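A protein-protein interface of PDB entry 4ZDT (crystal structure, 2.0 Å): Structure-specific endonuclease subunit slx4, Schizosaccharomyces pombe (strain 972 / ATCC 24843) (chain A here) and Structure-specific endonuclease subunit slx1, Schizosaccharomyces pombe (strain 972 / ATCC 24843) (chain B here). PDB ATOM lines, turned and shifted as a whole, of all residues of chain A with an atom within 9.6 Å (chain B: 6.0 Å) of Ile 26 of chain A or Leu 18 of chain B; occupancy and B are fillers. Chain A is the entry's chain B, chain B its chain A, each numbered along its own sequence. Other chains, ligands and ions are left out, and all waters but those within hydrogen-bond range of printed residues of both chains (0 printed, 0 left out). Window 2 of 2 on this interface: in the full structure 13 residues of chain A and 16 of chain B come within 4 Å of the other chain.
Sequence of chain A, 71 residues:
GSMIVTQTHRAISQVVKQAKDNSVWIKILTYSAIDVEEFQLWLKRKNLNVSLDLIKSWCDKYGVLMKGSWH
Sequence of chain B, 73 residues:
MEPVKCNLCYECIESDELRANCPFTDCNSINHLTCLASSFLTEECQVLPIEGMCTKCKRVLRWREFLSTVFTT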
ATOM      1  N   VAL A  16       0.160  26.678 -26.058  1.00  0.00           N
ATOM      2  CA  VAL A  16       1.540  26.745 -26.526  1.00  0.00           C
ATOM      3  C   VAL A  16       2.473  25.959 -25.604  1.00  0.00           C
ATOM      4  O   VAL A  16       3.325  25.204 -26.087  1.00  0.00           O
ATOM      5  CB  VAL A  16       2.005  28.230 -26.650  1.00  0.00           C
ATOM      6  CG1 VAL A  16       3.525  28.324 -26.895  1.00  0.00           C
ATOM      7  CG2 VAL A  16       1.232  28.907 -27.784  1.00  0.00           C
ATOM      8  N   LYS A  17       2.291  26.131 -24.298  1.00  0.00           N
ATOM      9  CA  LYS A  17       3.172  25.583 -23.282  1.00  0.00           C
ATOM     10  C   LYS A  17       2.838  24.156 -22.862  1.00  0.00           C
ATOM     11  O   LYS A  17       3.694  23.454 -22.309  1.00  0.00           O
ATOM     12  CB  LYS A  17       3.191  26.488 -22.043  1.00  0.00           C
ATOM     13  CG  LYS A  17       3.837  27.852 -22.309  1.00  0.00           C
ATOM     14  CD  LYS A  17       4.036  28.654 -21.035  1.00  0.00           C
ATOM     15  CE  LYS A  17       2.725  29.170 -20.455  1.00  0.00           C
ATOM     16  NZ  LYS A  17       3.006  30.025 -19.240  1.00  0.00           N
ATOM     17  N   ALA A  19       0.931  21.772 -25.015  1.00  0.00           N
ATOM     18  CA  ALA A  19       0.847  20.850 -26.143  1.00  0.00           C
ATOM     19  C   ALA A  19       2.078  19.942 -26.203  1.00  0.00           C
ATOM     20  O   ALA A  19       3.204  20.406 -25.950  1.00  0.00           O
ATOM     21  CB  ALA A  19       0.730  21.625 -27.440  1.00  0.00           C
ATOM     22  N   LYS A  20       1.872  18.669 -26.560  1.00  0.00           N
ATOM     23  CA  LYS A  20       3.004  17.746 -26.802  1.00  0.00           C
ATOM     24  C   LYS A  20       3.887  18.269 -27.919  1.00  0.00           C
ATOM     25  O   LYS A  20       5.097  18.088 -27.887  1.00  0.00           O
ATOM     26  CB  LYS A  20       2.536  16.324 -27.157  1.00  0.00           C
ATOM     27  CG  LYS A  20       1.499  15.732 -26.202  1.00  0.00           C
ATOM     28  CD  LYS A  20       2.064  15.323 -24.838  1.00  0.00           C
ATOM     29  CE  LYS A  20       0.981  14.639 -23.993  1.00  0.00           C
ATOM     30  NZ  LYS A  20       1.490  14.192 -22.669  1.00  0.00           N
ATOM     31  N   ASP A  21       3.272  18.902 -28.911  1.00  0.00           N
ATOM     32  CA  ASP A  21       4.001  19.559 -29.983  1.00  0.00           C
ATOM     33  C   ASP A  21       4.539  20.921 -29.493  1.00  0.00           C
ATOM     34  O   ASP A  21       3.801  21.919 -29.442  1.00  0.00           O
ATOM     35  CB  ASP A  21       3.095  19.740 -31.197  1.00  0.00           C
ATOM     36  CG  ASP A  21       3.757  20.514 -32.320  1.00  0.00           C
ATOM     37  OD1 ASP A  21       4.972  20.810 -32.272  1.00  0.00           O
ATOM     38  OD2 ASP A  21       3.054  20.831 -33.277  1.00  0.00           O
ATOM     39  N   ASN A  22       5.819  20.936 -29.122  1.00  0.00           N
ATOM     40  CA  ASN A  22       6.433  22.123 -28.529  1.00  0.00           C
ATOM     41  C   ASN A  22       7.081  23.061 -29.541  1.00  0.00           C
ATOM     42  O   ASN A  22       7.779  24.023 -29.166  1.00  0.00           O
ATOM     43  CB  ASN A  22       7.424  21.718 -27.422  1.00  0.00           C
ATOM     44  CG  ASN A  22       8.694  21.070 -27.961  1.00  0.00           C
ATOM     45  OD1 ASN A  22       8.881  20.928 -29.167  1.00  0.00           O
ATOM     46  ND2 ASN A  22       9.573  20.671 -27.049  1.00  0.00           N
ATOM     47  N   SER A  23       6.852  22.784 -30.820  1.00  0.00           N
ATOM     48  CA  SER A  23       7.500  23.520 -31.894  1.00  0.00           C
ATOM     49  C   SER A  23       7.133  24.999 -31.897  1.00  0.00           C
ATOM     50  O   SER A  23       7.982  25.842 -32.208  1.00  0.00           O
ATOM     51  CB  SER A  23       7.224  22.883 -33.263  1.00  0.00           C
ATOM     52  OG  SER A  23       5.832  22.837 -33.560  1.00  0.00           O
ATOM     53  N   VAL A  24       5.881  25.324 -31.570  1.00  0.00           N
ATOM     54  CA  VAL A  24       5.498  26.733 -31.508  1.00  0.00           C
ATOM     55  C   VAL A  24       6.246  27.427 -30.370  1.00  0.00           C
ATOM     56  O   VAL A  24       6.747  28.527 -30.542  1.00  0.00           O
ATOM     57  CB  VAL A  24       3.972  26.953 -31.336  1.00  0.00           C
ATOM     58  CG1 VAL A  24       3.666  28.446 -31.119  1.00  0.00           C
ATOM     59  CG2 VAL A  24       3.221  26.441 -32.545  1.00  0.00           C
ATOM     60  N   TRP A  25       6.287  26.800 -29.201  1.00  0.00           N
ATOM     61  CA  TRP A  25       6.956  27.432 -28.075  1.00  0.00           C
ATOM     62  C   TRP A  25       8.437  27.640 -28.430  1.00  0.00           C
ATOM     63  O   TRP A  25       9.004  28.697 -28.153  1.00  0.00           O
ATOM     64  CB  TRP A  25       6.784  26.631 -26.793  1.00  0.00           C
ATOM     65  CG  TRP A  25       7.076  27.429 -25.545  1.00  0.00           C
ATOM     66  CD1 TRP A  25       7.314  28.783 -25.461  1.00  0.00           C
ATOM     67  CD2 TRP A  25       7.111  26.938 -24.213  1.00  0.00           C
ATOM     68  NE1 TRP A  25       7.513  29.150 -24.159  1.00  0.00           N
ATOM     69  CE2 TRP A  25       7.399  28.036 -23.369  1.00  0.00           C
ATOM     70  CE3 TRP A  25       6.935  25.669 -23.640  1.00  0.00           C
ATOM     71  CZ2 TRP A  25       7.509  27.906 -21.985  1.00  0.00           C
ATOM     72  CZ3 TRP A  25       7.036  25.539 -22.269  1.00  0.00           C
ATOM     73  CH2 TRP A  25       7.331  26.649 -21.451  1.00  0.00           C
ATOM     74  N   ILE A  26       9.037  26.649 -29.089  1.00  0.00           N
ATOM     75  CA  ILE A  26      10.456  26.741 -29.470  1.00  0.00           C
ATOM     76  C   ILE A  26      10.700  27.884 -30.453  1.00  0.00           C
ATOM     77  O   ILE A  26      11.726  28.565 -30.375  1.00  0.00           O
ATOM     78  CB  ILE A  26      10.969  25.400 -30.042  1.00  0.00           C
ATOM     79  CG1 ILE A  26      10.961  24.325 -28.944  1.00  0.00           C
ATOM     80  CG2 ILE A  26      12.372  25.558 -30.652  1.00  0.00           C
ATOM     81  CD1 ILE A  26      12.045  24.493 -27.928  1.00  0.00           C
ATOM     82  N   LYS A  27       9.753  28.114 -31.367  1.00  0.00           N
ATOM     83  CA  LYS A  27       9.852  29.267 -32.261  1.00  0.00           C
ATOM     84  C   LYS A  27       9.881  30.578 -31.473  1.00  0.00           C
ATOM     85  O   LYS A  27      10.751  31.431 -31.697  1.00  0.00           O
ATOM     86  CB  LYS A  27       8.705  29.286 -33.299  1.00  0.00           C
ATOM     87  CG  LYS A  27       8.925  28.300 -34.465  1.00  0.00           C
ATOM     88  CD  LYS A  27       7.722  28.314 -35.416  1.00  0.00           C
ATOM     89  CE  LYS A  27       7.895  27.327 -36.562  1.00  0.00           C
ATOM     90  NZ  LYS A  27       6.776  27.500 -37.504  1.00  0.00           N
ATOM     91  N   ILE A  28       8.942  30.724 -30.548  1.00  0.00           N
ATOM     92  CA  ILE A  28       8.827  31.910 -29.694  1.00  0.00           C
ATOM     93  C   ILE A  28      10.119  32.118 -28.896  1.00  0.00           C
ATOM     94  O   ILE A  28      10.655  33.224 -28.843  1.00  0.00           O
ATOM     95  CB  ILE A  28       7.623  31.769 -28.717  1.00  0.00           C
ATOM     96  CG1 ILE A  28       6.298  31.801 -29.507  1.00  0.00           C
ATOM     97  CG2 ILE A  28       7.633  32.868 -27.600  1.00  0.00           C
ATOM     98  CD1 ILE A  28       5.071  31.352 -28.686  1.00  0.00           C
ATOM     99  N   LEU A  29      10.602  31.043 -28.283  1.00  0.00           N
ATOM    100  CA  LEU A  29      11.804  31.102 -27.446  1.00  0.00           C
ATOM    101  C   LEU A  29      13.089  31.412 -28.223  1.00  0.00           C
ATOM    102  O   LEU A  29      14.117  31.726 -27.617  1.00  0.00           O
ATOM    103  CB  LEU A  29      11.958  29.800 -26.648  1.00  0.00           C
ATOM    104  CG  LEU A  29      10.863  29.478 -25.628  1.00  0.00           C
ATOM    105  CD1 LEU A  29      11.070  28.065 -25.024  1.00  0.00           C
ATOM    106  CD2 LEU A  29      10.787  30.538 -24.521  1.00  0.00           C
ATOM    107  N   THR A  30      13.042  31.289 -29.544  1.00  0.00           N
ATOM    108  CA  THR A  30      14.200  31.560 -30.393  1.00  0.00           C
ATOM    109  C   THR A  30      13.964  32.768 -31.294  1.00  0.00           C
ATOM    110  O   THR A  30      14.690  32.978 -32.262  1.00  0.00           O
ATOM    111  CB  THR A  30      14.619  30.326 -31.225  1.00  0.00           C
ATOM    112  OG1 THR A  30      13.555  29.945 -32.102  1.00  0.00           O
ATOM    113  CG2 THR A  30      14.952  29.152 -30.306  1.00  0.00           C
ATOM    114  N   TYR A  31      12.955  33.568 -30.946  1.00  0.00           N
ATOM    115  CA  TYR A  31      12.596  34.779 -31.694  1.00  0.00           C
ATOM    116  C   TYR A  31      12.311  34.520 -33.189  1.00  0.00           C
ATOM    117  O   TYR A  31      12.629  35.357 -34.036  1.00  0.00           O
ATOM    118  CB  TYR A  31      13.690  35.877 -31.523  1.00  0.00           C
ATOM    119  CG  TYR A  31      14.011  36.181 -30.058  1.00  0.00           C
ATOM    120  CD1 TYR A  31      13.182  37.022 -29.319  1.00  0.00           C
ATOM    121  CD2 TYR A  31      15.124  35.631 -29.432  1.00  0.00           C
ATOM    122  CE1 TYR A  31      13.455  37.301 -27.995  1.00  0.00           C
ATOM    123  CE2 TYR A  31      15.413  35.910 -28.106  1.00  0.00           C
ATOM    124  CZ  TYR A  31      14.583  36.732 -27.393  1.00  0.00           C
ATOM    125  OH  TYR A  31      14.864  36.999 -26.074  1.00  0.00           O
ATOM    126  N   SER A  32      11.724  33.347 -33.496  1.00  0.00           N
ATOM    127  CA  SER A  32      11.302  33.014 -34.866  1.00  0.00           C
ATOM    128  C   SER A  32       9.844  33.363 -35.105  1.00  0.00           C
ATOM    129  O   SER A  32       8.968  33.023 -34.296  1.00  0.00           O
ATOM    130  CB  SER A  32      11.505  31.516 -35.178  1.00  0.00           C
ATOM    131  OG  SER A  32      12.821  31.100 -34.866  1.00  0.00           O
ATOM    132  N   ALA A  33       9.589  34.011 -36.241  1.00  0.00           N
ATOM    133  CA  ALA A  33       8.239  34.473 -36.598  1.00  0.00           C
ATOM    134  C   ALA A  33       7.239  33.342 -36.806  1.00  0.00           C
ATOM    135  O   ALA A  33       7.574  32.268 -37.311  1.00  0.00           O
ATOM    136  CB  ALA A  33       8.279  35.353 -37.818  1.00  0.00           C
ATOM    137  N   ILE A  34       6.001  33.632 -36.422  1.00  0.00           N
ATOM    138  CA  ILE A  34       4.873  32.713 -36.448  1.00  0.00           C
ATOM    139  C   ILE A  34       3.937  33.109 -37.596  1.00  0.00           C
ATOM    140  O   ILE A  34       3.704  34.292 -37.803  1.00  0.00           O
ATOM    141  CB  ILE A  34       4.161  32.798 -35.050  1.00  0.00           C
ATOM    142  CG1 ILE A  34       5.160  32.475 -33.914  1.00  0.00           C
ATOM    143  CG2 ILE A  34       2.887  31.975 -34.962  1.00  0.00           C
ATOM    144  CD1 ILE A  34       5.793  31.098 -34.008  1.00  0.00           C
ATOM    145  N   TRP A  42      -3.461  25.469 -36.054  1.00  0.00           N
ATOM    146  CA  TRP A  42      -2.740  24.664 -35.059  1.00  0.00           C
ATOM    147  C   TRP A  42      -3.496  24.696 -33.730  1.00  0.00           C
ATOM    148  O   TRP A  42      -3.725  23.659 -33.109  1.00  0.00           O
ATOM    149  CB  TRP A  42      -1.309  25.204 -34.895  1.00  0.00           C
ATOM    150  CG  TRP A  42      -0.358  24.422 -33.975  1.00  0.00           C
ATOM    151  CD1 TRP A  42       0.468  23.389 -34.336  1.00  0.00           C
ATOM    152  CD2 TRP A  42      -0.087  24.680 -32.587  1.00  0.00           C
ATOM    153  NE1 TRP A  42       1.211  22.963 -33.248  1.00  0.00           N
ATOM    154  CE2 TRP A  42       0.891  23.739 -32.166  1.00  0.00           C
ATOM    155  CE3 TRP A  42      -0.578  25.612 -31.654  1.00  0.00           C
ATOM    156  CZ2 TRP A  42       1.385  23.700 -30.852  1.00  0.00           C
ATOM    157  CZ3 TRP A  42      -0.085  25.570 -30.339  1.00  0.00           C
ATOM    158  CH2 TRP A  42       0.888  24.614 -29.956  1.00  0.00           C
ATOM    159  N   VAL A  64       5.574  37.713 -29.448  1.00  0.00           N
ATOM    160  CA  VAL A  64       5.654  36.737 -30.524  1.00  0.00           C
ATOM    161  C   VAL A  64       5.675  37.491 -31.862  1.00  0.00           C
ATOM    162  O   VAL A  64       4.836  38.374 -32.087  1.00  0.00           O
ATOM    163  CB  VAL A  64       4.473  35.758 -30.427  1.00  0.00           C
ATOM    164  CG1 VAL A  64       4.489  34.741 -31.573  1.00  0.00           C
ATOM    165  CG2 VAL A  64       4.485  35.063 -29.043  1.00  0.00           C
ATOM    166  N   ILE B  13      19.248  15.112 -23.902  1.00  0.00           N
ATOM    167  CA  ILE B  13      19.081  16.086 -24.968  1.00  0.00           C
ATOM    168  C   ILE B  13      19.706  15.493 -26.218  1.00  0.00           C
ATOM    169  O   ILE B  13      20.907  15.261 -26.266  1.00  0.00           O
ATOM    170  CB  ILE B  13      19.731  17.462 -24.621  1.00  0.00           C
ATOM    171  CG1 ILE B  13      19.161  18.012 -23.308  1.00  0.00           C
ATOM    172  CG2 ILE B  13      19.525  18.456 -25.758  1.00  0.00           C
ATOM    173  CD1 ILE B  13      19.853  19.282 -22.797  1.00  0.00           C
ATOM    174  N   GLU B  14      18.873  15.256 -27.225  1.00  0.00           N
ATOM    175  CA  GLU B  14      19.309  14.635 -28.473  1.00  0.00           C
ATOM    176  C   GLU B  14      20.305  15.526 -29.212  1.00  0.00           C
ATOM    177  O   GLU B  14      20.426  16.716 -28.905  1.00  0.00           O
ATOM    178  CB  GLU B  14      18.103  14.309 -29.368  1.00  0.00           C
ATOM    179  CG  GLU B  14      17.036  13.401 -28.726  1.00  0.00           C
ATOM    180  CD  GLU B  14      17.586  12.065 -28.216  1.00  0.00           C
ATOM    181  OE1 GLU B  14      18.611  11.574 -28.751  1.00  0.00           O
ATOM    182  OE2 GLU B  14      16.984  11.503 -27.274  1.00  0.00           O
ATOM    183  N   ASP B  16      20.165  16.457 -32.342  1.00  0.00           N
ATOM    184  CA  ASP B  16      19.452  17.337 -33.270  1.00  0.00           C
ATOM    185  C   ASP B  16      18.654  18.422 -32.546  1.00  0.00           C
ATOM    186  O   ASP B  16      18.002  19.265 -33.181  1.00  0.00           O
ATOM    187  CB  ASP B  16      18.514  16.511 -34.162  1.00  0.00           C
ATOM    188  CG  ASP B  16      19.270  15.619 -35.144  1.00  0.00           C
ATOM    189  OD1 ASP B  16      20.423  15.958 -35.506  1.00  0.00           O
ATOM    190  OD2 ASP B  16      18.702  14.583 -35.563  1.00  0.00           O
ATOM    191  N   GLU B  17      18.711  18.395 -31.217  1.00  0.00           N
ATOM    192  CA  GLU B  17      17.851  19.234 -30.399  1.00  0.00           C
ATOM    193  C   GLU B  17      18.559  20.528 -30.007  1.00  0.00           C
ATOM    194  O   GLU B  17      19.744  20.518 -29.677  1.00  0.00           O
ATOM    195  CB  GLU B  17      17.422  18.468 -29.149  1.00  0.00           C
ATOM    196  CG  GLU B  17      16.042  18.829 -28.645  1.00  0.00           C
ATOM    197  CD  GLU B  17      15.546  17.899 -27.557  1.00  0.00           C
ATOM    198  OE1 GLU B  17      14.425  18.127 -27.056  1.00  0.00           O
ATOM    199  OE2 GLU B  17      16.266  16.940 -27.200  1.00  0.00           O
ATOM    200  N   LEU B  18      17.821  21.634 -30.056  1.00  0.00           N
ATOM    201  CA  LEU B  18      18.301  22.910 -29.542  1.00  0.00           C
ATOM    202  C   LEU B  18      18.366  22.845 -28.019  1.00  0.00           C
ATOM    203  O   LEU B  18      17.585  22.133 -27.386  1.00  0.00           O
ATOM    204  CB  LEU B  18      17.382  24.048 -29.981  1.00  0.00           C
ATOM    205  CG  LEU B  18      17.182  24.281 -31.476  1.00  0.00           C
ATOM    206  CD1 LEU B  18      16.142  25.376 -31.712  1.00  0.00           C
ATOM    207  CD2 LEU B  18      18.507  24.611 -32.208  1.00  0.00           C
ATOM    208  N   ARG B  19      19.292  23.590 -27.425  1.00  0.00           N
ATOM    209  CA  ARG B  19      19.450  23.582 -25.968  1.00  0.00           C
ATOM    210  C   ARG B  19      20.062  24.866 -25.416  1.00  0.00           C
ATOM    211  O   ARG B  19      20.972  25.442 -26.014  1.00  0.00           O
ATOM    212  CB  ARG B  19      20.284  22.375 -25.530  1.00  0.00           C
ATOM    213  CG  ARG B  19      21.785  22.588 -25.633  1.00  0.00           C
ATOM    214  CD  ARG B  19      22.492  21.322 -26.088  1.00  0.00           C
ATOM    215  NE  ARG B  19      21.896  20.768 -27.303  1.00  0.00           N
ATOM    216  CZ  ARG B  19      22.222  19.591 -27.835  1.00  0.00           C
ATOM    217  NH1 ARG B  19      23.161  18.848 -27.252  1.00  0.00           N
ATOM    218  NH2 ARG B  19      21.628  19.165 -28.942  1.00  0.00           N
ATOM    219  N   ALA B  20      19.558  25.303 -24.266  1.00  0.00           N
ATOM    220  CA  ALA B  20      20.092  26.471 -23.582  1.00  0.00           C
ATOM    221  C   ALA B  20      21.403  26.104 -22.915  1.00  0.00           C
ATOM    222  O   ALA B  20      21.568  24.968 -22.440  1.00  0.00           O
ATOM    223  CB  ALA B  20      19.110  26.964 -22.542  1.00  0.00           C
ATOM    224  N   ASN B  31      20.557  22.881 -20.528  1.00  0.00           N
ATOM    225  CA  ASN B  31      19.177  22.450 -20.322  1.00  0.00           C
ATOM    226  C   ASN B  31      18.276  22.706 -21.528  1.00  0.00           C
ATOM    227  O   ASN B  31      18.605  23.509 -22.402  1.00  0.00           O
ATOM    228  CB  ASN B  31      18.589  23.120 -19.077  1.00  0.00           C
ATOM    229  CG  ASN B  31      19.060  24.551 -18.909  1.00  0.00           C
ATOM    230  OD1 ASN B  31      18.918  25.374 -19.813  1.00  0.00           O
ATOM    231  ND2 ASN B  31      19.624  24.855 -17.746  1.00  0.00           N
ATOM    232  N   HIS B  32      17.135  22.018 -21.568  1.00  0.00           N
ATOM    233  CA  HIS B  32      16.164  22.182 -22.660  1.00  0.00           C
ATOM    234  C   HIS B  32      15.694  23.626 -22.631  1.00  0.00           C
ATOM    235  O   HIS B  32      15.522  24.191 -21.558  1.00  0.00           O
ATOM    236  CB  HIS B  32      14.914  21.312 -22.443  1.00  0.00           C
ATOM    237  CG  HIS B  32      15.125  19.853 -22.675  1.00  0.00           C
ATOM    238  ND1 HIS B  32      15.142  18.932 -21.645  1.00  0.00           N
ATOM    239  CD2 HIS B  32      15.296  19.147 -23.817  1.00  0.00           C
ATOM    240  CE1 HIS B  32      15.325  17.722 -22.150  1.00  0.00           C
ATOM    241  NE2 HIS B  32      15.419  17.826 -23.463  1.00  0.00           N
ATOM    242  N   LEU B  33      15.484  24.214 -23.807  1.00  0.00           N
ATOM    243  CA  LEU B  33      14.906  25.568 -23.896  1.00  0.00           C
ATOM    244  C   LEU B  33      13.616  25.676 -23.122  1.00  0.00           C
ATOM    245  O   LEU B  33      13.447  26.600 -22.333  1.00  0.00           O
ATOM    246  CB  LEU B  33      14.648  25.968 -25.354  1.00  0.00           C
ATOM    247  CG  LEU B  33      15.872  26.123 -26.255  1.00  0.00           C
ATOM    248  CD1 LEU B  33      15.441  26.250 -27.712  1.00  0.00           C
ATOM    249  CD2 LEU B  33      16.663  27.387 -25.817  1.00  0.00           C
ATOM    250  N   THR B  34      12.695  24.728 -23.349  1.00  0.00           N
ATOM    251  CA  THR B  34      11.398  24.795 -22.680  1.00  0.00           C
ATOM    252  C   THR B  34      11.534  24.644 -21.178  1.00  0.00           C
ATOM    253  O   THR B  34      10.885  25.367 -20.432  1.00  0.00           O
ATOM    254  CB  THR B  34      10.371  23.785 -23.256  1.00  0.00           C
ATOM    255  OG1 THR B  34      10.954  22.479 -23.255  1.00  0.00           O
ATOM    256  CG2 THR B  34      10.045  24.154 -24.672  1.00  0.00           C
ATOM    257  N   THR B  69      24.150  28.765 -28.807  1.00  0.00           N
ATOM    258  CA  THR B  69      24.344  27.712 -29.791  1.00  0.00           C
ATOM    259  C   THR B  69      23.150  27.567 -30.719  1.00  0.00           C
ATOM    260  O   THR B  69      23.184  26.785 -31.663  1.00  0.00           O
ATOM    261  CB  THR B  69      24.667  26.358 -29.131  1.00  0.00           C
ATOM    262  OG1 THR B  69      23.532  25.902 -28.369  1.00  0.00           O
ATOM    263  CG2 THR B  69      25.917  26.491 -28.195  1.00  0.00           C
ATOM    264  N   VAL B  70      22.096  28.335 -30.460  1.00  0.00           N
ATOM    265  CA  VAL B  70      20.844  28.176 -31.197  1.00  0.00           C
ATOM    266  C   VAL B  70      20.933  28.668 -32.655  1.00  0.00           C
ATOM    267  O   VAL B  70      20.393  28.030 -33.583  1.00  0.00           O
ATOM    268  CB  VAL B  70      19.707  28.867 -30.422  1.00  0.00           C
ATOM    269  CG1 VAL B  70      18.521  29.185 -31.323  1.00  0.00           C
ATOM    270  CG2 VAL B  70      19.310  27.996 -29.234  1.00  0.00           C
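Of the printed residues of chain B, Trp 25 of chain A touches Thr 34.
Of chain B, only Leu 18 (3.9 Å), Leu 33 (3.8 Å) and Thr 34 (3.8 Å) come within 4 Å of Ile 26 of chain A.
Of the printed residues of chain B, Leu 29 of chain A touches Leu 33 (3.9 Å).
Of the printed residues of chain B, Thr 30 of chain A touches Leu 33 (3.9 Å) and Val 70 (3.7 Å).
No residue of chain A comes within 4 Å of Glu 17 of chain B.
Leu 18 of chain B touches just one residue of chain A: Ile 26 (3.9 Å).
Of the printed residues of chain A, Leu 33 of chain B touches Ile 26 (3.8 Å), Leu 29 (3.9 Å) and Thr 30 (3.9 Å).
Printed residues of chain A within 4 Å of Thr 34 of chain B: Trp 25 (3.6 Å) and Ile 26 (3.8 Å).
Val 70 of chain B touches just one residue of chain A: Thr 30.
The nearest printed residue of chain A that does not touch Leu 33 of chain B is Trp 25 of chain A (6.1 Å).
OG1 of Thr 30 of chain A lies within hydrogen-bond range of O of Ile 26 of chain A (2.9 Å).
The backbone carbonyl oxygen of Lys 27 of chain A is in hydrogen-bond range of the side-chain hydroxyl of Thr 30 of chain A (3.2 Å).
The side-chain hydroxyl (OG) of Ser 32 of chain A lies within hydrogen-bond range of the side-chain hydroxyl (OG1) of Thr 30 of chain A, at 3.1 Å.
Printed residues of chain B that touch a printed residue of chain A: Leu 18, Leu 33, Thr 34 and Val 70.
Hydrophobic or aromatic side chains of chain B within 4 Å of the printed part of chain A: Leu 18, Leu 33 and Val 70.
Among the printed residues, no Asp or Glu carboxylate lies within 4 Å of a Lys or Arg side-chain nitrogen of the other chain.
Trp 25 of chain A touches Thr 34 of chain B.
CG2 of Ile 26 of chain A touches CD1 of Leu 18 of chain B (3.9 Å).
Ile 26 of chain A touches Leu 33 of chain B (CD1 to CD1, 3.8 Å).
Ile 26 of chain A touches Thr 34 of chain B (CD1 to CG2, 3.8 Å).
Leu 29 of chain A touches Leu 33 of chain B.
Leu 33 of chain B touches Thr 30 of chain A (CD1 to CG2, 3.9 Å).
Val 70 of chain B touches Thr 30 of chain A.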
